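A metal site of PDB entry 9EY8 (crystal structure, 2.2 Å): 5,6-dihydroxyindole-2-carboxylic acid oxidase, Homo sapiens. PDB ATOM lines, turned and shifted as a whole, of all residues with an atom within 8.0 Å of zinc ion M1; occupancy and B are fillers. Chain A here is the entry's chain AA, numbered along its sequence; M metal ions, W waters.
Zinc ion M1 is bound by water W1 (2.0 Å), NE2 of His 191 (2.2 Å), NE2 of His 200 (2.2 Å) and NE2 of His 168 (2.2 Å). Zinc ion M1 has four donor atoms within binding distance.
ND1 of His 191 lies within hydrogen-bond range of OG of Ser 190 (3.0 Å). The side-chain carboxylate (OD1) of Asp 188 is in hydrogen-bond range of the backbone NH (N) of His 191, at 2.9 Å. A ring nitrogen (ND1) of His 200 sits at hydrogen-bond distance from the backbone carbonyl oxygen (O) of Phe 196. A ring nitrogen (ND1) of His 168 lies close to the backbone carbonyl oxygen (O) of Thr 367, 3.4 Å away. O of His 168 is in hydrogen-bond range of OG of Ser 171 (2.8 Å).
Phe 376 touches zinc ion M1.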
ATOM      1  N   HIS A 168      -1.126  10.348 -28.606  1.00  0.00           N
ATOM      2  CA  HIS A 168      -1.293  10.206 -27.168  1.00  0.00           C
ATOM      3  C   HIS A 168       0.031  10.362 -26.432  1.00  0.00           C
ATOM      4  O   HIS A 168       0.125  11.160 -25.482  1.00  0.00           O
ATOM      5  CB  HIS A 168      -1.915   8.845 -26.884  1.00  0.00           C
ATOM      6  CG  HIS A 168      -2.484   8.738 -25.505  1.00  0.00           C
ATOM      7  ND1 HIS A 168      -1.793   8.161 -24.453  1.00  0.00           N
ATOM      8  CD2 HIS A 168      -3.642   9.191 -24.993  1.00  0.00           C
ATOM      9  CE1 HIS A 168      -2.520   8.246 -23.364  1.00  0.00           C
ATOM     10  NE2 HIS A 168      -3.652   8.865 -23.660  1.00  0.00           N
ATOM     11  N   TYR A 169       1.070   9.637 -26.852  1.00  0.00           N
ATOM     12  CA  TYR A 169       2.390   9.768 -26.230  1.00  0.00           C
ATOM     13  C   TYR A 169       2.883  11.207 -26.265  1.00  0.00           C
ATOM     14  O   TYR A 169       3.468  11.701 -25.292  1.00  0.00           O
ATOM     15  CB  TYR A 169       3.415   8.850 -26.922  1.00  0.00           C
ATOM     16  CG  TYR A 169       4.811   9.465 -26.892  1.00  0.00           C
ATOM     17  CD1 TYR A 169       5.648   9.273 -25.803  1.00  0.00           C
ATOM     18  CD2 TYR A 169       5.274  10.277 -27.946  1.00  0.00           C
ATOM     19  CE1 TYR A 169       6.910   9.887 -25.738  1.00  0.00           C
ATOM     20  CE2 TYR A 169       6.549  10.888 -27.884  1.00  0.00           C
ATOM     21  CZ  TYR A 169       7.356  10.673 -26.779  1.00  0.00           C
ATOM     22  OH  TYR A 169       8.618  11.255 -26.713  1.00  0.00           O
ATOM     23  N   SER A 171       1.237  14.037 -26.407  1.00  0.00           N
ATOM     24  CA  SER A 171       0.497  14.940 -25.547  1.00  0.00           C
ATOM     25  C   SER A 171       0.876  14.774 -24.083  1.00  0.00           C
ATOM     26  O   SER A 171       0.627  15.709 -23.311  1.00  0.00           O
ATOM     27  CB  SER A 171      -0.998  14.716 -25.719  1.00  0.00           C
ATOM     28  OG  SER A 171      -1.407  13.491 -25.126  1.00  0.00           O
ATOM     29  N   VAL A 172       1.450  13.645 -23.665  1.00  0.00           N
ATOM     30  CA  VAL A 172       1.769  13.438 -22.255  1.00  0.00           C
ATOM     31  C   VAL A 172       3.251  13.518 -21.946  1.00  0.00           C
ATOM     32  O   VAL A 172       3.612  13.551 -20.756  1.00  0.00           O
ATOM     33  CB  VAL A 172       1.215  12.096 -21.721  1.00  0.00           C
ATOM     34  CG1 VAL A 172      -0.234  11.883 -22.164  1.00  0.00           C
ATOM     35  CG2 VAL A 172       2.097  10.950 -22.133  1.00  0.00           C
ATOM     36  N   ASP A 188       0.980  17.949 -19.020  1.00  0.00           N
ATOM     37  CA  ASP A 188       0.221  16.879 -19.651  1.00  0.00           C
ATOM     38  C   ASP A 188      -0.922  17.547 -20.388  1.00  0.00           C
ATOM     39  O   ASP A 188      -1.824  18.127 -19.769  1.00  0.00           O
ATOM     40  CB  ASP A 188      -0.261  15.855 -18.608  1.00  0.00           C
ATOM     41  CG  ASP A 188      -0.866  14.606 -19.237  1.00  0.00           C
ATOM     42  OD1 ASP A 188      -1.566  14.720 -20.278  1.00  0.00           O
ATOM     43  OD2 ASP A 188      -0.651  13.484 -18.685  1.00  0.00           O
ATOM     44  N   SER A 190      -3.304  16.338 -22.150  1.00  0.00           N
ATOM     45  CA  SER A 190      -4.529  15.569 -22.351  1.00  0.00           C
ATOM     46  C   SER A 190      -5.080  14.933 -21.089  1.00  0.00           C
ATOM     47  O   SER A 190      -6.107  14.236 -21.182  1.00  0.00           O
ATOM     48  CB  SER A 190      -4.303  14.482 -23.403  1.00  0.00           C
ATOM     49  OG  SER A 190      -3.155  13.722 -23.042  1.00  0.00           O
ATOM     50  N   HIS A 191      -4.446  15.130 -19.932  1.00  0.00           N
ATOM     51  CA  HIS A 191      -4.893  14.580 -18.658  1.00  0.00           C
ATOM     52  C   HIS A 191      -4.731  15.618 -17.561  1.00  0.00           C
ATOM     53  O   HIS A 191      -3.975  16.582 -17.705  1.00  0.00           O
ATOM     54  CB  HIS A 191      -4.071  13.330 -18.246  1.00  0.00           C
ATOM     55  CG  HIS A 191      -4.098  12.260 -19.254  1.00  0.00           C
ATOM     56  ND1 HIS A 191      -3.402  12.316 -20.443  1.00  0.00           N
ATOM     57  CD2 HIS A 191      -4.811  11.101 -19.298  1.00  0.00           C
ATOM     58  CE1 HIS A 191      -3.648  11.235 -21.156  1.00  0.00           C
ATOM     59  NE2 HIS A 191      -4.491  10.480 -20.475  1.00  0.00           N
ATOM     60  N   PHE A 196      -9.237  16.821 -20.616  1.00  0.00           N
ATOM     61  CA  PHE A 196      -9.152  15.360 -20.634  1.00  0.00           C
ATOM     62  C   PHE A 196     -10.281  14.734 -21.459  1.00  0.00           C
ATOM     63  O   PHE A 196     -10.047  13.835 -22.291  1.00  0.00           O
ATOM     64  CB  PHE A 196      -9.181  14.787 -19.224  1.00  0.00           C
ATOM     65  CG  PHE A 196      -9.500  13.340 -19.172  1.00  0.00           C
ATOM     66  CD1 PHE A 196      -8.530  12.383 -19.489  1.00  0.00           C
ATOM     67  CD2 PHE A 196     -10.761  12.903 -18.796  1.00  0.00           C
ATOM     68  CE1 PHE A 196      -8.797  11.036 -19.436  1.00  0.00           C
ATOM     69  CE2 PHE A 196     -11.076  11.558 -18.759  1.00  0.00           C
ATOM     70  CZ  PHE A 196     -10.083  10.607 -19.078  1.00  0.00           C
ATOM     71  N   TRP A 199     -10.205  16.093 -25.405  1.00  0.00           N
ATOM     72  CA  TRP A 199      -9.056  15.532 -26.122  1.00  0.00           C
ATOM     73  C   TRP A 199      -9.326  14.079 -26.491  1.00  0.00           C
ATOM     74  O   TRP A 199      -9.133  13.665 -27.640  1.00  0.00           O
ATOM     75  CB  TRP A 199      -7.794  15.657 -25.250  1.00  0.00           C
ATOM     76  CG  TRP A 199      -6.482  15.400 -25.974  1.00  0.00           C
ATOM     77  CD1 TRP A 199      -5.582  16.333 -26.378  1.00  0.00           C
ATOM     78  CD2 TRP A 199      -5.945  14.124 -26.372  1.00  0.00           C
ATOM     79  NE1 TRP A 199      -4.515  15.745 -26.985  1.00  0.00           N
ATOM     80  CE2 TRP A 199      -4.703  14.379 -26.990  1.00  0.00           C
ATOM     81  CE3 TRP A 199      -6.381  12.804 -26.242  1.00  0.00           C
ATOM     82  CZ2 TRP A 199      -3.886  13.357 -27.502  1.00  0.00           C
ATOM     83  CZ3 TRP A 199      -5.574  11.779 -26.735  1.00  0.00           C
ATOM     84  CH2 TRP A 199      -4.346  12.061 -27.372  1.00  0.00           C
ATOM     85  N   HIS A 200      -9.772  13.286 -25.533  1.00  0.00           N
ATOM     86  CA  HIS A 200      -9.965  11.882 -25.817  1.00  0.00           C
ATOM     87  C   HIS A 200     -11.164  11.650 -26.733  1.00  0.00           C
ATOM     88  O   HIS A 200     -11.188  10.650 -27.462  1.00  0.00           O
ATOM     89  CB  HIS A 200     -10.133  11.102 -24.512  1.00  0.00           C
ATOM     90  CG  HIS A 200      -8.839  10.858 -23.813  1.00  0.00           C
ATOM     91  ND1 HIS A 200      -8.206  11.809 -23.047  1.00  0.00           N
ATOM     92  CD2 HIS A 200      -8.041   9.765 -23.807  1.00  0.00           C
ATOM     93  CE1 HIS A 200      -7.085  11.312 -22.575  1.00  0.00           C
ATOM     94  NE2 HIS A 200      -6.967  10.063 -23.002  1.00  0.00           N
ATOM     95  N   HIS A 203      -9.654  12.206 -30.234  1.00  0.00           N
ATOM     96  CA  HIS A 203      -8.803  11.031 -30.421  1.00  0.00           C
ATOM     97  C   HIS A 203      -9.568   9.842 -31.031  1.00  0.00           C
ATOM     98  O   HIS A 203      -9.140   9.243 -32.033  1.00  0.00           O
ATOM     99  CB  HIS A 203      -8.244  10.656 -29.038  1.00  0.00           C
ATOM    100  CG  HIS A 203      -7.054   9.770 -29.076  1.00  0.00           C
ATOM    101  ND1 HIS A 203      -6.800   8.838 -28.091  1.00  0.00           N
ATOM    102  CD2 HIS A 203      -6.001   9.708 -29.928  1.00  0.00           C
ATOM    103  CE1 HIS A 203      -5.659   8.225 -28.354  1.00  0.00           C
ATOM    104  NE2 HIS A 203      -5.151   8.726 -29.463  1.00  0.00           N
ATOM    105  N   GLU A 336     -12.579  11.135 -14.783  1.00  0.00           N
ATOM    106  CA  GLU A 336     -11.186  10.809 -15.068  1.00  0.00           C
ATOM    107  C   GLU A 336     -10.637   9.866 -13.997  1.00  0.00           C
ATOM    108  O   GLU A 336      -9.921   8.902 -14.309  1.00  0.00           O
ATOM    109  CB  GLU A 336     -10.337  12.083 -15.200  1.00  0.00           C
ATOM    110  CG  GLU A 336      -8.905  11.794 -15.746  1.00  0.00           C
ATOM    111  CD  GLU A 336      -7.996  13.037 -15.880  1.00  0.00           C
ATOM    112  OE1 GLU A 336      -8.479  14.176 -15.714  1.00  0.00           O
ATOM    113  OE2 GLU A 336      -6.772  12.853 -16.160  1.00  0.00           O
ATOM    114  N   HIS A 353     -12.380   5.950 -14.751  1.00  0.00           N
ATOM    115  CA  HIS A 353     -11.483   5.741 -15.889  1.00  0.00           C
ATOM    116  C   HIS A 353     -10.056   5.375 -15.443  1.00  0.00           C
ATOM    117  O   HIS A 353      -9.430   4.466 -16.012  1.00  0.00           O
ATOM    118  CB  HIS A 353     -11.467   6.984 -16.786  1.00  0.00           C
ATOM    119  CG  HIS A 353     -10.131   7.282 -17.392  1.00  0.00           C
ATOM    120  ND1 HIS A 353      -9.159   7.985 -16.724  1.00  0.00           N
ATOM    121  CD2 HIS A 353      -9.593   6.942 -18.595  1.00  0.00           C
ATOM    122  CE1 HIS A 353      -8.093   8.087 -17.489  1.00  0.00           C
ATOM    123  NE2 HIS A 353      -8.335   7.473 -18.620  1.00  0.00           N
ATOM    124  N   ASN A 354      -9.515   6.084 -14.448  1.00  0.00           N
ATOM    125  CA  ASN A 354      -8.173   5.738 -13.974  1.00  0.00           C
ATOM    126  C   ASN A 354      -8.119   4.298 -13.458  1.00  0.00           C
ATOM    127  O   ASN A 354      -7.188   3.545 -13.782  1.00  0.00           O
ATOM    128  CB  ASN A 354      -7.721   6.705 -12.878  1.00  0.00           C
ATOM    129  CG  ASN A 354      -7.257   8.063 -13.397  1.00  0.00           C
ATOM    130  OD1 ASN A 354      -6.937   8.228 -14.574  1.00  0.00           O
ATOM    131  ND2 ASN A 354      -7.178   9.048 -12.496  1.00  0.00           N
ATOM    132  N   HIS A 357      -7.887   1.638 -16.100  1.00  0.00           N
ATOM    133  CA  HIS A 357      -6.520   1.479 -16.601  1.00  0.00           C
ATOM    134  C   HIS A 357      -5.668   0.617 -15.671  1.00  0.00           C
ATOM    135  O   HIS A 357      -4.958  -0.285 -16.122  1.00  0.00           O
ATOM    136  CB  HIS A 357      -5.841   2.845 -16.782  1.00  0.00           C
ATOM    137  CG  HIS A 357      -6.153   3.493 -18.074  1.00  0.00           C
ATOM    138  ND1 HIS A 357      -5.644   3.050 -19.276  1.00  0.00           N
ATOM    139  CD2 HIS A 357      -6.950   4.554 -18.371  1.00  0.00           C
ATOM    140  CE1 HIS A 357      -6.109   3.800 -20.258  1.00  0.00           C
ATOM    141  NE2 HIS A 357      -6.903   4.715 -19.738  1.00  0.00           N
ATOM    142  N   GLN A 366      -0.192   2.345 -18.129  1.00  0.00           N
ATOM    143  CA  GLN A 366       0.917   3.295 -18.104  1.00  0.00           C
ATOM    144  C   GLN A 366       0.616   4.399 -19.100  1.00  0.00           C
ATOM    145  O   GLN A 366       0.290   4.124 -20.271  1.00  0.00           O
ATOM    146  CB  GLN A 366       2.239   2.602 -18.439  1.00  0.00           C
ATOM    147  CG  GLN A 366       2.507   1.341 -17.642  1.00  0.00           C
ATOM    148  CD  GLN A 366       3.787   0.650 -18.086  1.00  0.00           C
ATOM    149  OE1 GLN A 366       3.784  -0.542 -18.422  1.00  0.00           O
ATOM    150  NE2 GLN A 366       4.885   1.396 -18.107  1.00  0.00           N
ATOM    151  N   THR A 367       0.735   5.646 -18.648  1.00  0.00           N
ATOM    152  CA  THR A 367       0.143   6.765 -19.364  1.00  0.00           C
ATOM    153  C   THR A 367       0.767   6.950 -20.743  1.00  0.00           C
ATOM    154  O   THR A 367       0.059   7.145 -21.735  1.00  0.00           O
ATOM    155  CB  THR A 367       0.276   8.056 -18.544  1.00  0.00           C
ATOM    156  OG1 THR A 367      -0.127   7.822 -17.191  1.00  0.00           O
ATOM    157  CG2 THR A 367      -0.586   9.175 -19.145  1.00  0.00           C
ATOM    158  N   HIS A 368       2.104   6.873 -20.843  1.00  0.00           N
ATOM    159  CA  HIS A 368       2.739   7.082 -22.140  1.00  0.00           C
ATOM    160  C   HIS A 368       2.555   5.897 -23.081  1.00  0.00           C
ATOM    161  O   HIS A 368       2.798   6.052 -24.286  1.00  0.00           O
ATOM    162  CB  HIS A 368       4.226   7.364 -21.959  1.00  0.00           C
ATOM    163  CG  HIS A 368       5.025   6.142 -21.633  1.00  0.00           C
ATOM    164  ND1 HIS A 368       4.884   5.456 -20.448  1.00  0.00           N
ATOM    165  CD2 HIS A 368       5.955   5.470 -22.357  1.00  0.00           C
ATOM    166  CE1 HIS A 368       5.706   4.411 -20.448  1.00  0.00           C
ATOM    167  NE2 HIS A 368       6.369   4.402 -21.592  1.00  0.00           N
ATOM    168  N   SER A 370      -0.390   3.512 -22.871  1.00  0.00           N
ATOM    169  CA  SER A 370      -1.622   2.736 -22.707  1.00  0.00           C
ATOM    170  C   SER A 370      -2.416   2.458 -23.983  1.00  0.00           C
ATOM    171  O   SER A 370      -3.068   1.398 -24.021  1.00  0.00           O
ATOM    172  CB  SER A 370      -2.537   3.407 -21.657  1.00  0.00           C
ATOM    173  OG  SER A 370      -2.926   4.693 -22.070  1.00  0.00           O
ATOM    174  N   PRO A 371      -2.458   3.324 -25.016  1.00  0.00           N
ATOM    175  CA  PRO A 371      -3.160   2.956 -26.265  1.00  0.00           C
ATOM    176  C   PRO A 371      -2.592   1.735 -26.971  1.00  0.00           C
ATOM    177  O   PRO A 371      -3.295   1.163 -27.809  1.00  0.00           O
ATOM    178  CB  PRO A 371      -3.014   4.206 -27.151  1.00  0.00           C
ATOM    179  CG  PRO A 371      -2.798   5.323 -26.177  1.00  0.00           C
ATOM    180  CD  PRO A 371      -1.941   4.707 -25.112  1.00  0.00           C
ATOM    181  N   PHE A 376      -7.738  -0.001 -24.823  1.00  0.00           N
ATOM    182  CA  PHE A 376      -7.805   1.458 -24.672  1.00  0.00           C
ATOM    183  C   PHE A 376      -8.987   2.057 -25.438  1.00  0.00           C
ATOM    184  O   PHE A 376      -9.718   2.896 -24.901  1.00  0.00           O
ATOM    185  CB  PHE A 376      -6.476   2.087 -25.148  1.00  0.00           C
ATOM    186  CG  PHE A 376      -6.401   3.604 -24.989  1.00  0.00           C
ATOM    187  CD1 PHE A 376      -6.980   4.450 -25.916  1.00  0.00           C
ATOM    188  CD2 PHE A 376      -5.749   4.161 -23.894  1.00  0.00           C
ATOM    189  CE1 PHE A 376      -6.930   5.830 -25.764  1.00  0.00           C
ATOM    190  CE2 PHE A 376      -5.674   5.533 -23.724  1.00  0.00           C
ATOM    191  CZ  PHE A 376      -6.256   6.375 -24.664  1.00  0.00           C
ATOM    192  N   LEU A 379     -12.216   1.175 -23.646  1.00  0.00           N
ATOM    193  CA  LEU A 379     -12.265   1.856 -22.365  1.00  0.00           C
ATOM    194  C   LEU A 379     -12.639   3.322 -22.549  1.00  0.00           C
ATOM    195  O   LEU A 379     -13.364   3.901 -21.732  1.00  0.00           O
ATOM    196  CB  LEU A 379     -10.913   1.693 -21.654  1.00  0.00           C
ATOM    197  CG  LEU A 379     -10.619   2.173 -20.231  1.00  0.00           C
ATOM    198  CD1 LEU A 379      -9.370   1.467 -19.663  1.00  0.00           C
ATOM    199  CD2 LEU A 379     -10.469   3.725 -20.129  1.00  0.00           C
ATOM    200  N   HIS A 380     -12.190   3.935 -23.664  1.00  0.00           N
ATOM    201  CA  HIS A 380     -12.442   5.352 -23.881  1.00  0.00           C
ATOM    202  C   HIS A 380     -13.716   5.658 -24.642  1.00  0.00           C
ATOM    203  O   HIS A 380     -14.228   6.777 -24.485  1.00  0.00           O
ATOM    204  CB  HIS A 380     -11.257   5.997 -24.593  1.00  0.00           C
ATOM    205  CG  HIS A 380     -10.292   6.573 -23.632  1.00  0.00           C
ATOM    206  ND1 HIS A 380     -10.615   7.677 -22.861  1.00  0.00           N
ATOM    207  CD2 HIS A 380      -9.090   6.132 -23.186  1.00  0.00           C
ATOM    208  CE1 HIS A 380      -9.612   7.921 -22.025  1.00  0.00           C
ATOM    209  NE2 HIS A 380      -8.671   7.013 -22.233  1.00  0.00           N
HETATM  210 ZN    ZN M   1      -5.185   9.175 -22.058  1.00  0.00          ZN
HETATM  211 ZN    ZN M   2      -7.366   6.738 -20.492  1.00  0.00          ZN
HETATM  212  O   HOH W   1      -5.712   7.602 -20.891  1.00  0.00           O
